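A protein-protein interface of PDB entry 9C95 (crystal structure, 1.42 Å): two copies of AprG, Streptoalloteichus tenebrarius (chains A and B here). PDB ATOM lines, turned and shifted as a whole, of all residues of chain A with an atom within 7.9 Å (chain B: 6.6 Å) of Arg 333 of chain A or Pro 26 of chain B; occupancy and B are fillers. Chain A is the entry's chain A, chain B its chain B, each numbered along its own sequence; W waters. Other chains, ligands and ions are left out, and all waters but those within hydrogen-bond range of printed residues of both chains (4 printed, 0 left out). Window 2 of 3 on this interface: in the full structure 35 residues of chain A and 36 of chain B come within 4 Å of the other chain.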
ATOM      1  N   TYR A 266      17.457  19.553 -36.283  1.00  0.00           N
ATOM      2  CA  TYR A 266      17.600  19.624 -34.838  1.00  0.00           C
ATOM      3  C   TYR A 266      16.798  18.531 -34.150  1.00  0.00           C
ATOM      4  O   TYR A 266      17.333  17.804 -33.307  1.00  0.00           O
ATOM      5  CB  TYR A 266      17.174  20.999 -34.315  1.00  0.00           C
ATOM      6  CG  TYR A 266      17.231  21.058 -32.797  1.00  0.00           C
ATOM      7  CD1 TYR A 266      18.452  20.866 -32.120  1.00  0.00           C
ATOM      8  CD2 TYR A 266      16.090  21.262 -32.052  1.00  0.00           C
ATOM      9  CE1 TYR A 266      18.507  20.879 -30.756  1.00  0.00           C
ATOM     10  CE2 TYR A 266      16.122  21.292 -30.653  1.00  0.00           C
ATOM     11  CZ  TYR A 266      17.362  21.092 -30.015  1.00  0.00           C
ATOM     12  OH  TYR A 266      17.417  21.139 -28.634  1.00  0.00           O
ATOM     13  N   ARG A 267      15.525  18.347 -34.533  1.00  0.00           N
ATOM     14  CA  ARG A 267      14.760  17.281 -33.903  1.00  0.00           C
ATOM     15  C   ARG A 267      15.414  15.921 -34.117  1.00  0.00           C
ATOM     16  O   ARG A 267      15.449  15.107 -33.194  1.00  0.00           O
ATOM     17  CB  ARG A 267      13.312  17.239 -34.399  1.00  0.00           C
ATOM     18  CG  ARG A 267      12.535  16.115 -33.728  1.00  0.00           C
ATOM     19  CD  ARG A 267      11.071  16.203 -33.956  1.00  0.00           C
ATOM     20  NE  ARG A 267      10.677  16.224 -35.361  1.00  0.00           N
ATOM     21  CZ  ARG A 267      10.529  15.179 -36.170  1.00  0.00           C
ATOM     22  NH1 ARG A 267      10.797  13.949 -35.778  1.00  0.00           N
ATOM     23  NH2 ARG A 267      10.101  15.385 -37.403  1.00  0.00           N
ATOM     24  N   ARG A 326       6.884  23.397 -34.501  1.00  0.00           N
ATOM     25  CA  ARG A 326       6.647  22.059 -33.972  1.00  0.00           C
ATOM     26  C   ARG A 326       7.916  21.222 -33.887  1.00  0.00           C
ATOM     27  O   ARG A 326       8.058  20.456 -32.927  1.00  0.00           O
ATOM     28  CB  ARG A 326       5.486  21.368 -34.645  1.00  0.00           C
ATOM     29  CG  ARG A 326       5.812  20.902 -35.981  1.00  0.00           C
ATOM     30  CD  ARG A 326       4.473  20.731 -36.673  1.00  0.00           C
ATOM     31  NE  ARG A 326       4.554  19.794 -37.751  1.00  0.00           N
ATOM     32  CZ  ARG A 326       3.685  19.720 -38.763  1.00  0.00           C
ATOM     33  NH1 ARG A 326       3.822  18.766 -39.662  1.00  0.00           N
ATOM     34  NH2 ARG A 326       2.724  20.610 -38.930  1.00  0.00           N
ATOM     35  N   ASN A 327       8.851  21.375 -34.839  1.00  0.00           N
ATOM     36  CA  ASN A 327      10.107  20.631 -34.741  1.00  0.00           C
ATOM     37  C   ASN A 327      11.015  21.168 -33.650  1.00  0.00           C
ATOM     38  O   ASN A 327      11.703  20.375 -32.998  1.00  0.00           O
ATOM     39  CB  ASN A 327      10.809  20.559 -36.088  1.00  0.00           C
ATOM     40  CG  ASN A 327      10.134  19.579 -37.010  1.00  0.00           C
ATOM     41  OD1 ASN A 327      10.178  18.384 -36.785  1.00  0.00           O
ATOM     42  ND2 ASN A 327       9.513  20.074 -38.066  1.00  0.00           N
ATOM     43  N   LEU A 328      11.015  22.485 -33.409  1.00  0.00           N
ATOM     44  CA  LEU A 328      11.767  23.021 -32.271  1.00  0.00           C
ATOM     45  C   LEU A 328      11.179  22.570 -30.942  1.00  0.00           C
ATOM     46  O   LEU A 328      11.930  22.228 -30.020  1.00  0.00           O
ATOM     47  CB  LEU A 328      11.842  24.549 -32.317  1.00  0.00           C
ATOM     48  CG  LEU A 328      12.732  25.115 -33.413  1.00  0.00           C
ATOM     49  CD1 LEU A 328      12.823  26.637 -33.345  1.00  0.00           C
ATOM     50  CD2 LEU A 328      14.147  24.529 -33.326  1.00  0.00           C
ATOM     51  N   ALA A 329       9.860  22.563 -30.803  1.00  0.00           N
ATOM     52  CA  ALA A 329       9.260  22.180 -29.525  1.00  0.00           C
ATOM     53  C   ALA A 329       9.513  20.703 -29.234  1.00  0.00           C
ATOM     54  O   ALA A 329       9.899  20.334 -28.108  1.00  0.00           O
ATOM     55  CB  ALA A 329       7.759  22.467 -29.558  1.00  0.00           C
ATOM     56  N   SER A 330       9.342  19.843 -30.241  1.00  0.00           N
ATOM     57  CA  SER A 330       9.623  18.423 -30.037  1.00  0.00           C
ATOM     58  C   SER A 330      11.116  18.169 -29.889  1.00  0.00           C
ATOM     59  O   SER A 330      11.510  17.305 -29.090  1.00  0.00           O
ATOM     60  CB  SER A 330       9.029  17.581 -31.178  1.00  0.00           C
ATOM     61  OG  SER A 330       7.607  17.471 -31.041  1.00  0.00           O
ATOM     62  N   GLY A 331      11.948  18.912 -30.622  1.00  0.00           N
ATOM     63  CA  GLY A 331      13.392  18.796 -30.439  1.00  0.00           C
ATOM     64  C   GLY A 331      13.827  19.115 -29.022  1.00  0.00           C
ATOM     65  O   GLY A 331      14.697  18.439 -28.462  1.00  0.00           O
ATOM     66  N   GLU A 332      13.248  20.160 -28.420  1.00  0.00           N
ATOM     67  CA  GLU A 332      13.536  20.462 -27.020  1.00  0.00           C
ATOM     68  C   GLU A 332      13.121  19.311 -26.111  1.00  0.00           C
ATOM     69  O   GLU A 332      13.857  18.919 -25.194  1.00  0.00           O
ATOM     70  CB  GLU A 332      12.809  21.744 -26.609  1.00  0.00           C
ATOM     71  CG  GLU A 332      13.062  22.148 -25.152  1.00  0.00           C
ATOM     72  CD  GLU A 332      12.154  23.262 -24.647  1.00  0.00           C
ATOM     73  OE1 GLU A 332      11.021  23.396 -25.148  1.00  0.00           O
ATOM     74  OE2 GLU A 332      12.582  23.999 -23.724  1.00  0.00           O
ATOM     75  N   ARG A 333      11.928  18.762 -26.345  1.00  0.00           N
ATOM     76  CA  ARG A 333      11.486  17.637 -25.529  1.00  0.00           C
ATOM     77  C   ARG A 333      12.458  16.467 -25.629  1.00  0.00           C
ATOM     78  O   ARG A 333      12.772  15.834 -24.610  1.00  0.00           O
ATOM     79  CB  ARG A 333      10.073  17.209 -25.953  1.00  0.00           C
ATOM     80  CG  ARG A 333       9.530  15.993 -25.192  1.00  0.00           C
ATOM     81  CD  ARG A 333       8.048  15.658 -25.564  1.00  0.00           C
ATOM     82  NE  ARG A 333       7.156  16.685 -25.066  1.00  0.00           N
ATOM     83  CZ  ARG A 333       6.652  17.656 -25.823  1.00  0.00           C
ATOM     84  NH1 ARG A 333       5.882  18.586 -25.267  1.00  0.00           N
ATOM     85  NH2 ARG A 333       6.934  17.730 -27.137  1.00  0.00           N
ATOM     86  N   VAL A 334      12.949  16.170 -26.831  1.00  0.00           N
ATOM     87  CA  VAL A 334      13.814  15.003 -27.032  1.00  0.00           C
ATOM     88  C   VAL A 334      15.225  15.248 -26.495  1.00  0.00           C
ATOM     89  O   VAL A 334      15.799  14.371 -25.820  1.00  0.00           O
ATOM     90  CB  VAL A 334      13.836  14.580 -28.518  1.00  0.00           C
ATOM     91  CG1 VAL A 334      14.972  13.578 -28.790  1.00  0.00           C
ATOM     92  CG2 VAL A 334      12.462  14.013 -28.966  1.00  0.00           C
ATOM     93  N   TRP A 335      15.802  16.432 -26.751  1.00  0.00           N
ATOM     94  CA  TRP A 335      17.240  16.640 -26.557  1.00  0.00           C
ATOM     95  C   TRP A 335      17.610  17.544 -25.399  1.00  0.00           C
ATOM     96  O   TRP A 335      18.778  17.524 -24.989  1.00  0.00           O
ATOM     97  CB  TRP A 335      17.889  17.250 -27.812  1.00  0.00           C
ATOM     98  CG  TRP A 335      17.804  16.372 -29.009  1.00  0.00           C
ATOM     99  CD1 TRP A 335      16.936  16.487 -30.046  1.00  0.00           C
ATOM    100  CD2 TRP A 335      18.604  15.217 -29.286  1.00  0.00           C
ATOM    101  NE1 TRP A 335      17.141  15.494 -30.957  1.00  0.00           N
ATOM    102  CE2 TRP A 335      18.158  14.684 -30.508  1.00  0.00           C
ATOM    103  CE3 TRP A 335      19.672  14.578 -28.616  1.00  0.00           C
ATOM    104  CZ2 TRP A 335      18.735  13.574 -31.102  1.00  0.00           C
ATOM    105  CZ3 TRP A 335      20.250  13.455 -29.199  1.00  0.00           C
ATOM    106  CH2 TRP A 335      19.784  12.963 -30.432  1.00  0.00           C
ATOM    107  N   ALA A 336      16.696  18.357 -24.889  1.00  0.00           N
ATOM    108  CA  ALA A 336      17.131  19.408 -23.958  1.00  0.00           C
ATOM    109  C   ALA A 336      16.866  19.054 -22.508  1.00  0.00           C
ATOM    110  O   ALA A 336      16.263  18.025 -22.206  1.00  0.00           O
ATOM    111  CB  ALA A 336      16.507  20.774 -24.317  1.00  0.00           C
ATOM    112  N   GLN B  24      -2.731  19.016 -21.633  1.00  0.00           N
ATOM    113  CA  GLN B  24      -1.727  18.067 -22.095  1.00  0.00           C
ATOM    114  C   GLN B  24      -0.556  18.036 -21.123  1.00  0.00           C
ATOM    115  O   GLN B  24      -0.143  19.070 -20.597  1.00  0.00           O
ATOM    116  CB  GLN B  24      -1.220  18.486 -23.479  1.00  0.00           C
ATOM    117  CG  GLN B  24      -0.307  17.427 -24.104  1.00  0.00           C
ATOM    118  CD  GLN B  24      -0.039  17.720 -25.574  1.00  0.00           C
ATOM    119  OE1 GLN B  24       0.032  18.884 -25.989  1.00  0.00           O
ATOM    120  NE2 GLN B  24       0.088  16.690 -26.357  1.00  0.00           N
ATOM    121  N   ARG B  25      -0.017  16.835 -20.907  1.00  0.00           N
ATOM    122  CA  ARG B  25       1.074  16.590 -19.979  1.00  0.00           C
ATOM    123  C   ARG B  25       2.430  16.855 -20.633  1.00  0.00           C
ATOM    124  O   ARG B  25       2.551  16.904 -21.858  1.00  0.00           O
ATOM    125  CB  ARG B  25       0.959  15.155 -19.467  1.00  0.00           C
ATOM    126  CG  ARG B  25      -0.204  15.056 -18.467  1.00  0.00           C
ATOM    127  CD  ARG B  25      -0.759  13.657 -18.280  1.00  0.00           C
ATOM    128  NE  ARG B  25      -1.931  13.699 -17.401  1.00  0.00           N
ATOM    129  CZ  ARG B  25      -2.726  12.665 -17.131  1.00  0.00           C
ATOM    130  NH1 ARG B  25      -2.501  11.475 -17.669  1.00  0.00           N
ATOM    131  NH2 ARG B  25      -3.775  12.835 -16.326  1.00  0.00           N
ATOM    132  N   PRO B  26       3.484  17.043 -19.826  1.00  0.00           N
ATOM    133  CA  PRO B  26       4.777  17.447 -20.405  1.00  0.00           C
ATOM    134  C   PRO B  26       5.351  16.442 -21.381  1.00  0.00           C
ATOM    135  O   PRO B  26       6.018  16.838 -22.344  1.00  0.00           O
ATOM    136  CB  PRO B  26       5.677  17.627 -19.166  1.00  0.00           C
ATOM    137  CG  PRO B  26       4.684  17.947 -18.052  1.00  0.00           C
ATOM    138  CD  PRO B  26       3.488  17.104 -18.353  1.00  0.00           C
ATOM    139  N   ASN B  27       5.128  15.149 -21.165  1.00  0.00           N
ATOM    140  CA  ASN B  27       5.604  14.165 -22.113  1.00  0.00           C
ATOM    141  C   ASN B  27       4.751  14.078 -23.369  1.00  0.00           C
ATOM    142  O   ASN B  27       5.082  13.294 -24.254  1.00  0.00           O
ATOM    143  CB  ASN B  27       5.736  12.782 -21.446  1.00  0.00           C
ATOM    144  CG  ASN B  27       4.401  12.155 -21.099  1.00  0.00           C
ATOM    145  OD1 ASN B  27       3.365  12.821 -21.081  1.00  0.00           O
ATOM    146  ND2 ASN B  27       4.433  10.868 -20.736  1.00  0.00           N
ATOM    147  N   GLY B  28       3.682  14.863 -23.480  1.00  0.00           N
ATOM    148  CA  GLY B  28       2.791  14.782 -24.624  1.00  0.00           C
ATOM    149  C   GLY B  28       1.516  13.975 -24.413  1.00  0.00           C
ATOM    150  O   GLY B  28       0.610  14.036 -25.264  1.00  0.00           O
ATOM    151  N   ALA B  29       1.398  13.211 -23.326  1.00  0.00           N
ATOM    152  CA  ALA B  29       0.183  12.426 -23.151  1.00  0.00           C
ATOM    153  C   ALA B  29      -1.027  13.334 -22.888  1.00  0.00           C
ATOM    154  O   ALA B  29      -0.910  14.433 -22.345  1.00  0.00           O
ATOM    155  CB  ALA B  29       0.365  11.443 -21.988  1.00  0.00           C
ATOM    156  N   GLN B  54       1.828  21.642 -32.503  1.00  0.00           N
ATOM    157  CA  GLN B  54       2.816  21.365 -31.457  1.00  0.00           C
ATOM    158  C   GLN B  54       2.280  20.342 -30.468  1.00  0.00           C
ATOM    159  O   GLN B  54       2.989  19.404 -30.081  1.00  0.00           O
ATOM    160  CB  GLN B  54       3.244  22.654 -30.754  1.00  0.00           C
ATOM    161  CG  GLN B  54       4.225  23.440 -31.647  1.00  0.00           C
ATOM    162  CD  GLN B  54       4.456  24.868 -31.207  1.00  0.00           C
ATOM    163  OE1 GLN B  54       4.504  25.155 -30.009  1.00  0.00           O
ATOM    164  NE2 GLN B  54       4.607  25.781 -32.188  1.00  0.00           N
ATOM    165  N   SER B  57       2.341  16.999 -32.262  1.00  0.00           N
ATOM    166  CA  SER B  57       3.717  16.500 -32.301  1.00  0.00           C
ATOM    167  C   SER B  57       4.169  16.015 -30.940  1.00  0.00           C
ATOM    168  O   SER B  57       4.902  15.025 -30.869  1.00  0.00           O
ATOM    169  CB  SER B  57       4.632  17.624 -32.784  1.00  0.00           C
ATOM    170  OG  SER B  57       4.306  17.982 -34.122  1.00  0.00           O
ATOM    171  N   ALA B  58       3.692  16.617 -29.860  1.00  0.00           N
ATOM    172  CA  ALA B  58       3.977  16.108 -28.522  1.00  0.00           C
ATOM    173  C   ALA B  58       3.349  14.739 -28.286  1.00  0.00           C
ATOM    174  O   ALA B  58       3.990  13.859 -27.677  1.00  0.00           O
ATOM    175  CB  ALA B  58       3.562  17.133 -27.460  1.00  0.00           C
ATOM    176  N   VAL B  59       2.121  14.515 -28.783  1.00  0.00           N
ATOM    177  CA  VAL B  59       1.563  13.167 -28.761  1.00  0.00           C
ATOM    178  C   VAL B  59       2.460  12.230 -29.547  1.00  0.00           C
ATOM    179  O   VAL B  59       2.728  11.099 -29.114  1.00  0.00           O
ATOM    180  CB  VAL B  59       0.097  13.123 -29.255  1.00  0.00           C
ATOM    181  CG1 VAL B  59      -0.424  11.670 -29.157  1.00  0.00           C
ATOM    182  CG2 VAL B  59      -0.803  14.075 -28.405  1.00  0.00           C
ATOM    183  N   ASP B  61       5.636  12.444 -29.955  1.00  0.00           N
ATOM    184  CA  ASP B  61       6.817  12.137 -29.142  1.00  0.00           C
ATOM    185  C   ASP B  61       6.511  11.044 -28.124  1.00  0.00           C
ATOM    186  O   ASP B  61       7.330  10.132 -27.907  1.00  0.00           O
ATOM    187  CB  ASP B  61       7.305  13.402 -28.422  1.00  0.00           C
ATOM    188  CG  ASP B  61       7.740  14.516 -29.382  1.00  0.00           C
ATOM    189  OD1 ASP B  61       8.231  14.190 -30.463  1.00  0.00           O
ATOM    190  OD2 ASP B  61       7.568  15.725 -29.051  1.00  0.00           O
ATOM    191  N   TYR B  62       5.365  11.131 -27.454  1.00  0.00           N
ATOM    192  CA  TYR B  62       4.960  10.115 -26.484  1.00  0.00           C
ATOM    193  C   TYR B  62       4.805   8.766 -27.178  1.00  0.00           C
ATOM    194  O   TYR B  62       5.359   7.746 -26.747  1.00  0.00           O
ATOM    195  CB  TYR B  62       3.637  10.545 -25.839  1.00  0.00           C
ATOM    196  CG  TYR B  62       3.017   9.535 -24.881  1.00  0.00           C
ATOM    197  CD1 TYR B  62       3.729   9.069 -23.791  1.00  0.00           C
ATOM    198  CD2 TYR B  62       1.716   9.070 -25.066  1.00  0.00           C
ATOM    199  CE1 TYR B  62       3.175   8.169 -22.903  1.00  0.00           C
ATOM    200  CE2 TYR B  62       1.156   8.158 -24.177  1.00  0.00           C
ATOM    201  CZ  TYR B  62       1.894   7.717 -23.096  1.00  0.00           C
ATOM    202  OH  TYR B  62       1.353   6.796 -22.185  1.00  0.00           O
ATOM    203  N   ARG B 103       5.758  12.652 -39.853  1.00  0.00           N
ATOM    204  CA  ARG B 103       6.636  11.761 -39.082  1.00  0.00           C
ATOM    205  C   ARG B 103       6.735  10.436 -39.840  1.00  0.00           C
ATOM    206  O   ARG B 103       6.140   9.423 -39.467  1.00  0.00           O
ATOM    207  CB  ARG B 103       6.098  11.543 -37.669  1.00  0.00           C
ATOM    208  CG  ARG B 103       6.058  12.812 -36.776  1.00  0.00           C
ATOM    209  CD  ARG B 103       7.400  13.071 -36.194  1.00  0.00           C
ATOM    210  NE  ARG B 103       7.380  14.156 -35.200  1.00  0.00           N
ATOM    211  CZ  ARG B 103       7.610  13.985 -33.893  1.00  0.00           C
ATOM    212  NH1 ARG B 103       7.884  12.780 -33.384  1.00  0.00           N
ATOM    213  NH2 ARG B 103       7.575  15.053 -33.097  1.00  0.00           N
HETATM  214  O   HOH W   1       3.680  24.681 -34.688  1.00  0.00           O
HETATM  215  O   HOH W   2       5.881  19.458 -29.637  1.00  0.00           O
HETATM  216  O   HOH W   3       7.877  17.804 -34.605  1.00  0.00           O
HETATM  217  O   HOH W   4       3.325  19.232 -23.507  1.00  0.00           O
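The side-chain carboxylate (OD2) of Asp 61 of chain B sits at hydrogen-bond distance from the side-chain hydroxyl (OG) of Ser 330 of chain A.
The guanidinium group (NE) of Arg 333 of chain A is in hydrogen-bond range of the backbone carbonyl oxygen (O) of Pro 26 of chain B (3.0 Å).
The guanidinium group (NH1) of Arg 267 of chain A sits close to the guanidinium group (NE) of Arg 103 of chain B, at 3.5 Å.
The side-chain hydroxyl of Ser 330 of chain A lies within hydrogen-bond range of the guanidinium group of Arg 103 of chain B, 3.2 Å away.
The side-chain carboxylate (OD2) of Asp 61 of chain B lies within salt-bridge range of the guanidinium group (NH2) of Arg 333 of chain A.
The side-chain carboxylate (OD1) of Asp 61 of chain B is in salt-bridge range of the guanidinium group (NH2) of Arg 103 of chain B (2.8 Å).
The side-chain amide oxygen (OD1) of Asn 327 of chain A is in hydrogen-bond range of the guanidinium group (NE) of Arg 267 of chain A (2.6 Å).
O of Arg 267 of chain A sits at hydrogen-bond distance from NE1 of Trp 335 of chain A (2.8 Å).
N of Ala 29 of chain B lies within hydrogen-bond range of OD1 of Asn 27 of chain B.
The backbone carbonyl oxygen (O) of Ser 57 of chain B lies within hydrogen-bond range of the guanidinium group (NH2) of Arg 103 of chain B, at 3.5 Å.
Arg 326 of chain A touches Gln 54 of chain B.
Ser 57 of chain B touches Arg 326 of chain A (OG to CB, 3.6 Å).
CB of Ser 57 of chain B touches OG of Ser 330 of chain A, 3.5 Å away.
Arg 333 of chain A touches Asn 27 of chain B (NE to C, 3.9 Å).
NH2 of Arg 333 of chain A touches CB of Ala 58 of chain B (3.4 Å).
Arg 333 of chain A touches four residues of chain B.
Of chain A, only Arg 333 (3.0 Å) comes within 4 Å of Pro 26 of chain B.
Printed residues of chain A within 4 Å of Arg 103 of chain B: Arg 267 and Ser 330.
Printed residues of chain A within 4 Å of Asp 61 of chain B: Ser 330 (2.6 Å) and Arg 333 (2.8 Å).
Printed residues of chain A within 4 Å of Ala 58 of chain B: Arg 333 (3.4 Å).
Of the printed residues of chain B, Ser 330 of chain A touches Ser 57 (3.5 Å), Asp 61 (2.6 Å) and Arg 103 (3.2 Å).
The nearest residue of chain B that does not touch Arg 333 of chain A is Gly 28 of chain B (4.2 Å).
The nearest residue of chain A that does not touch Pro 26 of chain B is Ala 329 of chain A (7.8 Å).
Among the printed residues, 10 pairs touch across the chains.
Among the printed residues, Asp or Glu carboxylates within 4 Å of a Lys or Arg side-chain nitrogen of the other chain: Arg 333 of chain A with Asp 61 of chain B.
No position is printed for both chains.
Of the 10 pairs that touch across the chains among the printed residues, none has its exchanged pair printed and touching as well.
Water W1 bridges NE2 of Gln 54 of chain B and N of Arg 326 of chain A.
Water W2 lies within hydrogen-bond range of O of Gln 54 of chain B (2.9 Å), OG of Ser 330 of chain A (3.0 Å) and NH2 of Arg 333 of chain A (3.2 Å).
Water W4 lies within hydrogen-bond range of O of Arg 25 of chain B and NH1 of Arg 333 of chain A.
Water W3 lies within hydrogen-bond range of O of Arg 326 of chain A (3.1 Å), NH2 of Arg 103 of chain B (3.2 Å), OD1 of Asn 327 of chain A (3.2 Å) and NE of Arg 267 of chain A (3.3 Å).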
